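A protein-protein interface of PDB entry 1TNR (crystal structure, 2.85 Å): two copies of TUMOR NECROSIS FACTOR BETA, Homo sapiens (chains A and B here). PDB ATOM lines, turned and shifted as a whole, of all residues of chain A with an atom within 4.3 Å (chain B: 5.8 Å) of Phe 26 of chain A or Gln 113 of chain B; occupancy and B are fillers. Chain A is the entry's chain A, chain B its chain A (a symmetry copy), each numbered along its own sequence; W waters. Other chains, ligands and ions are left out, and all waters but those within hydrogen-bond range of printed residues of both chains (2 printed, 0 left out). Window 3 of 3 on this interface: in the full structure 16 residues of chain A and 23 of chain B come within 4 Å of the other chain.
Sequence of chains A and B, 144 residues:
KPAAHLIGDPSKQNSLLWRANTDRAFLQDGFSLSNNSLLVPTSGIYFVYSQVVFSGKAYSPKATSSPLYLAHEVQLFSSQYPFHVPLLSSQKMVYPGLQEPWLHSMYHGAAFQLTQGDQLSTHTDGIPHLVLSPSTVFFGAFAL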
ATOM      1  N   ALA A   3      16.538   7.608  30.368  1.00  0.00           N
ATOM      2  CA  ALA A   3      16.166   8.885  29.772  1.00  0.00           C
ATOM      3  C   ALA A   3      15.162   9.607  30.635  1.00  0.00           C
ATOM      4  O   ALA A   3      14.395   8.979  31.354  1.00  0.00           O
ATOM      5  CB  ALA A   3      15.585   8.671  28.395  1.00  0.00           C
ATOM      6  N   ALA A   4      15.154  10.927  30.541  1.00  0.00           N
ATOM      7  CA  ALA A   4      14.236  11.731  31.314  1.00  0.00           C
ATOM      8  C   ALA A   4      13.921  12.981  30.551  1.00  0.00           C
ATOM      9  O   ALA A   4      14.738  13.459  29.774  1.00  0.00           O
ATOM     10  CB  ALA A   4      14.835  12.095  32.647  1.00  0.00           C
ATOM     11  N   HIS A   5      12.692  13.452  30.732  1.00  0.00           N
ATOM     12  CA  HIS A   5      12.214  14.672  30.139  1.00  0.00           C
ATOM     13  C   HIS A   5      11.383  15.330  31.214  1.00  0.00           C
ATOM     14  O   HIS A   5      10.383  14.758  31.648  1.00  0.00           O
ATOM     15  CB  HIS A   5      11.311  14.418  28.948  1.00  0.00           C
ATOM     16  CG  HIS A   5      10.933  15.685  28.260  1.00  0.00           C
ATOM     17  ND1 HIS A   5      11.881  16.609  27.859  1.00  0.00           N
ATOM     18  CD2 HIS A   5       9.731  16.241  27.993  1.00  0.00           C
ATOM     19  CE1 HIS A   5      11.279  17.677  27.375  1.00  0.00           C
ATOM     20  NE2 HIS A   5       9.975  17.484  27.445  1.00  0.00           N
ATOM     21  N   ALA A  20       7.824  15.542  36.719  1.00  0.00           N
ATOM     22  CA  ALA A  20       7.650  14.537  35.696  1.00  0.00           C
ATOM     23  C   ALA A  20       6.323  13.785  35.696  1.00  0.00           C
ATOM     24  O   ALA A  20       6.179  12.773  35.005  1.00  0.00           O
ATOM     25  CB  ALA A  20       8.826  13.555  35.766  1.00  0.00           C
ATOM     26  N   ARG A  24       3.860  15.261  28.632  1.00  0.00           N
ATOM     27  CA  ARG A  24       4.736  14.232  28.087  1.00  0.00           C
ATOM     28  C   ARG A  24       6.069  14.042  28.843  1.00  0.00           C
ATOM     29  O   ARG A  24       7.026  13.468  28.316  1.00  0.00           O
ATOM     30  CB  ARG A  24       4.969  14.515  26.607  1.00  0.00           C
ATOM     31  CG  ARG A  24       3.706  14.457  25.772  1.00  0.00           C
ATOM     32  CD  ARG A  24       3.409  13.037  25.398  1.00  0.00           C
ATOM     33  NE  ARG A  24       2.094  12.880  24.778  1.00  0.00           N
ATOM     34  CZ  ARG A  24       1.615  11.709  24.330  1.00  0.00           C
ATOM     35  NH1 ARG A  24       2.345  10.600  24.424  1.00  0.00           N
ATOM     36  NH2 ARG A  24       0.408  11.625  23.775  1.00  0.00           N
ATOM     37  N   ALA A  25       6.131  14.495  30.089  1.00  0.00           N
ATOM     38  CA  ALA A  25       7.352  14.357  30.890  1.00  0.00           C
ATOM     39  C   ALA A  25       7.479  12.905  31.372  1.00  0.00           C
ATOM     40  O   ALA A  25       6.462  12.203  31.482  1.00  0.00           O
ATOM     41  CB  ALA A  25       7.298  15.321  32.079  1.00  0.00           C
ATOM     42  N   PHE A  26       8.700  12.455  31.672  1.00  0.00           N
ATOM     43  CA  PHE A  26       8.890  11.073  32.109  1.00  0.00           C
ATOM     44  C   PHE A  26      10.288  10.755  32.599  1.00  0.00           C
ATOM     45  O   PHE A  26      11.228  11.490  32.334  1.00  0.00           O
ATOM     46  CB  PHE A  26       8.578  10.114  30.969  1.00  0.00           C
ATOM     47  CG  PHE A  26       9.566  10.172  29.863  1.00  0.00           C
ATOM     48  CD1 PHE A  26       9.399  11.088  28.819  1.00  0.00           C
ATOM     49  CD2 PHE A  26      10.699   9.350  29.886  1.00  0.00           C
ATOM     50  CE1 PHE A  26      10.354  11.191  27.822  1.00  0.00           C
ATOM     51  CE2 PHE A  26      11.673   9.438  28.890  1.00  0.00           C
ATOM     52  CZ  PHE A  26      11.502  10.357  27.856  1.00  0.00           C
ATOM     53  N   LEU A  27      10.414   9.615  33.269  1.00  0.00           N
ATOM     54  CA  LEU A  27      11.673   9.117  33.797  1.00  0.00           C
ATOM     55  C   LEU A  27      11.644   7.630  33.522  1.00  0.00           C
ATOM     56  O   LEU A  27      10.585   7.006  33.642  1.00  0.00           O
ATOM     57  CB  LEU A  27      11.733   9.314  35.299  1.00  0.00           C
ATOM     58  CG  LEU A  27      11.677  10.744  35.809  1.00  0.00           C
ATOM     59  CD1 LEU A  27      11.165  10.689  37.206  1.00  0.00           C
ATOM     60  CD2 LEU A  27      13.067  11.393  35.784  1.00  0.00           C
ATOM     61  N   GLN A  28      12.758   7.063  33.079  1.00  0.00           N
ATOM     62  CA  GLN A  28      12.774   5.641  32.821  1.00  0.00           C
ATOM     63  C   GLN A  28      14.156   5.072  32.930  1.00  0.00           C
ATOM     64  O   GLN A  28      15.134   5.749  32.623  1.00  0.00           O
ATOM     65  CB  GLN A  28      12.209   5.322  31.451  1.00  0.00           C
ATOM     66  CG  GLN A  28      13.101   5.699  30.319  1.00  0.00           C
ATOM     67  CD  GLN A  28      12.761   4.897  29.070  1.00  0.00           C
ATOM     68  OE1 GLN A  28      11.592   4.642  28.773  1.00  0.00           O
ATOM     69  NE2 GLN A  28      13.775   4.469  28.351  1.00  0.00           N
ATOM     70  N   GLY B  44       8.143   3.931  21.042  1.00  0.00           N
ATOM     71  CA  GLY B  44       9.464   4.101  21.610  1.00  0.00           C
ATOM     72  C   GLY B  44       9.790   5.546  21.933  1.00  0.00           C
ATOM     73  O   GLY B  44       8.940   6.444  21.862  1.00  0.00           O
ATOM     74  N   ILE B  45      11.050   5.778  22.257  1.00  0.00           N
ATOM     75  CA  ILE B  45      11.491   7.116  22.591  1.00  0.00           C
ATOM     76  C   ILE B  45      12.185   7.757  21.425  1.00  0.00           C
ATOM     77  O   ILE B  45      13.140   7.205  20.876  1.00  0.00           O
ATOM     78  CB  ILE B  45      12.428   7.106  23.786  1.00  0.00           C
ATOM     79  CG1 ILE B  45      11.644   6.650  25.000  1.00  0.00           C
ATOM     80  CG2 ILE B  45      12.975   8.501  24.046  1.00  0.00           C
ATOM     81  CD1 ILE B  45      12.511   6.175  26.061  1.00  0.00           C
ATOM     82  N   TYR B  46      11.749   8.962  21.108  1.00  0.00           N
ATOM     83  CA  TYR B  46      12.299   9.693  19.987  1.00  0.00           C
ATOM     84  C   TYR B  46      12.772  11.078  20.349  1.00  0.00           C
ATOM     85  O   TYR B  46      12.199  11.748  21.217  1.00  0.00           O
ATOM     86  CB  TYR B  46      11.244   9.848  18.885  1.00  0.00           C
ATOM     87  CG  TYR B  46      10.863   8.559  18.184  1.00  0.00           C
ATOM     88  CD1 TYR B  46       9.914   7.685  18.735  1.00  0.00           C
ATOM     89  CD2 TYR B  46      11.417   8.228  16.949  1.00  0.00           C
ATOM     90  CE1 TYR B  46       9.529   6.515  18.058  1.00  0.00           C
ATOM     91  CE2 TYR B  46      11.034   7.067  16.267  1.00  0.00           C
ATOM     92  CZ  TYR B  46      10.092   6.217  16.820  1.00  0.00           C
ATOM     93  OH  TYR B  46       9.702   5.095  16.110  1.00  0.00           O
ATOM     94  N   ALA B 111      13.205  14.852  23.905  1.00  0.00           N
ATOM     95  CA  ALA B 111      12.897  13.428  23.780  1.00  0.00           C
ATOM     96  C   ALA B 111      11.493  13.082  24.309  1.00  0.00           C
ATOM     97  O   ALA B 111      11.092  13.557  25.386  1.00  0.00           O
ATOM     98  CB  ALA B 111      13.926  12.645  24.519  1.00  0.00           C
ATOM     99  N   PHE B 112      10.760  12.236  23.591  1.00  0.00           N
ATOM    100  CA  PHE B 112       9.414  11.876  24.028  1.00  0.00           C
ATOM    101  C   PHE B 112       9.123  10.412  23.822  1.00  0.00           C
ATOM    102  O   PHE B 112       9.809   9.722  23.056  1.00  0.00           O
ATOM    103  CB  PHE B 112       8.360  12.684  23.269  1.00  0.00           C
ATOM    104  CG  PHE B 112       8.580  14.183  23.312  1.00  0.00           C
ATOM    105  CD1 PHE B 112       8.084  14.949  24.377  1.00  0.00           C
ATOM    106  CD2 PHE B 112       9.278  14.832  22.279  1.00  0.00           C
ATOM    107  CE1 PHE B 112       8.280  16.340  24.407  1.00  0.00           C
ATOM    108  CE2 PHE B 112       9.478  16.222  22.298  1.00  0.00           C
ATOM    109  CZ  PHE B 112       8.981  16.981  23.362  1.00  0.00           C
ATOM    110  N   GLN B 113       8.148   9.922  24.580  1.00  0.00           N
ATOM    111  CA  GLN B 113       7.698   8.545  24.487  1.00  0.00           C
ATOM    112  C   GLN B 113       6.548   8.559  23.511  1.00  0.00           C
ATOM    113  O   GLN B 113       5.466   9.046  23.840  1.00  0.00           O
ATOM    114  CB  GLN B 113       7.205   8.046  25.830  1.00  0.00           C
ATOM    115  CG  GLN B 113       8.330   7.539  26.701  1.00  0.00           C
ATOM    116  CD  GLN B 113       7.879   7.177  28.111  1.00  0.00           C
ATOM    117  OE1 GLN B 113       6.922   7.762  28.649  1.00  0.00           O
ATOM    118  NE2 GLN B 113       8.581   6.216  28.728  1.00  0.00           N
ATOM    119  N   LEU B 114       6.805   8.101  22.294  1.00  0.00           N
ATOM    120  CA  LEU B 114       5.784   8.071  21.283  1.00  0.00           C
ATOM    121  C   LEU B 114       5.220   6.677  21.085  1.00  0.00           C
ATOM    122  O   LEU B 114       5.882   5.684  21.384  1.00  0.00           O
ATOM    123  CB  LEU B 114       6.377   8.551  19.981  1.00  0.00           C
ATOM    124  CG  LEU B 114       6.880   9.969  20.106  1.00  0.00           C
ATOM    125  CD1 LEU B 114       7.427  10.419  18.749  1.00  0.00           C
ATOM    126  CD2 LEU B 114       5.726  10.865  20.595  1.00  0.00           C
ATOM    127  N   THR B 115       4.032   6.622  20.498  1.00  0.00           N
ATOM    128  CA  THR B 115       3.334   5.381  20.186  1.00  0.00           C
ATOM    129  C   THR B 115       3.257   5.208  18.664  1.00  0.00           C
ATOM    130  O   THR B 115       3.075   6.183  17.929  1.00  0.00           O
ATOM    131  CB  THR B 115       1.913   5.479  20.713  1.00  0.00           C
ATOM    132  OG1 THR B 115       1.959   5.570  22.133  1.00  0.00           O
ATOM    133  CG2 THR B 115       1.077   4.306  20.292  1.00  0.00           C
ATOM    134  N   ASP B 118       1.328   7.609  15.923  1.00  0.00           N
ATOM    135  CA  ASP B 118       1.291   9.042  16.234  1.00  0.00           C
ATOM    136  C   ASP B 118       1.800   9.883  15.063  1.00  0.00           C
ATOM    137  O   ASP B 118       2.633   9.428  14.258  1.00  0.00           O
ATOM    138  CB  ASP B 118       2.194   9.359  17.416  1.00  0.00           C
ATOM    139  CG  ASP B 118       1.694   8.792  18.713  1.00  0.00           C
ATOM    140  OD1 ASP B 118       0.550   8.289  18.765  1.00  0.00           O
ATOM    141  OD2 ASP B 118       2.471   8.846  19.692  1.00  0.00           O
HETATM  142  O   HOH W   1       6.868  11.564  26.257  1.00  0.00           O
HETATM  143  O   HOH W   2       1.623   8.449  22.339  1.00  0.00           O
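OE1 of Gln 28 of chain A sits at hydrogen-bond distance from NE2 of Gln 113 of chain B.
O of Ala 3 of chain A sits at hydrogen-bond distance from N of Gln 28 of chain A, at 3.1 Å. O of Tyr 46 of chain B lies within hydrogen-bond range of N of Phe 112 of chain B (2.8 Å). N of Phe 26 of chain A lies within hydrogen-bond range of O of His 5 of chain A (2.9 Å).
His 5 of chain A touches Ala 111 of chain B. His 5 of chain A touches Phe 112 of chain B (NE2 to CE1, 3.7 Å). Phe 112 of chain B touches Arg 24 of chain A. Gln 113 of chain B touches Arg 24 of chain A (O to NH1, 3.5 Å). CE1 of Phe 26 of chain A touches O of Ala 111 of chain B, 3.5 Å away. Phe 112 of chain B touches Phe 26 of chain A (CA to CE1, 3.97 Å). CB of Phe 26 of chain A touches OE1 of Gln 113 of chain B, 3.7 Å away. NE2 of Gln 28 of chain A touches CD1 of Ile 45 of chain B, 3.1 Å away.
Ala 3 of chain A touches none of the printed residues of chain B. Printed residues of chain B within 4 Å of His 5 of chain A: Ala 111 and Phe 112. Printed residues of chain B within 4 Å of Arg 24 of chain A: Phe 112 and Gln 113. Ala 25 of chain A touches none of the printed residues of chain B. Phe 26 of chain A touches just these residues of chain B: Ala 111 (3.5 Å), Phe 112 (3.97 Å) and Gln 113 (3.7 Å). Printed residues of chain A within 4 Å of Phe 112 of chain B: His 5, Arg 24 and Phe 26. Of the printed residues of chain A, Gln 113 of chain B touches Arg 24, Phe 26 and Gln 28. The nearest printed residue of chain A that does not touch Gln 113 of chain B is Ala 25 of chain A (5.3 Å). The nearest printed residue of chain A that does not touch Phe 112 of chain B is Ala 25 of chain A (6.1 Å).
Printed residues of chain A that touch a printed residue of chain B: His 5, Arg 24, Phe 26 and Gln 28. Hydrophobic or aromatic side chains of chain A that line the printed part of chain B: His 5 and Phe 26. Printed residues of chain B that touch a printed residue of chain A: Ile 45, Ala 111, Phe 112 and Gln 113. Hydrophobic or aromatic side chains of chain B that line the printed part of chain A: Ile 45 and Phe 112. Among the printed residues, 9 pairs touch across the chains. Among the printed residues, no Asp or Glu carboxylate lies within 4 Å of a Lys or Arg side-chain nitrogen of the other chain.
No position is printed for both chains. Of the 9 pairs that touch across the chains among the printed residues, none has its exchanged pair printed and touching as well.
Water W1 bridges N of Gln 113 of chain B and O of Arg 24 of chain A. Water W2 lies within hydrogen-bond range of the side-chain carboxylate (OD2) of Asp 118 of chain B (2.8 Å), the side-chain hydroxyl (OG1) of Thr 115 of chain B (2.9 Å) and the guanidinium group (NH1) of Arg 24 of chain A (3.1 Å).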
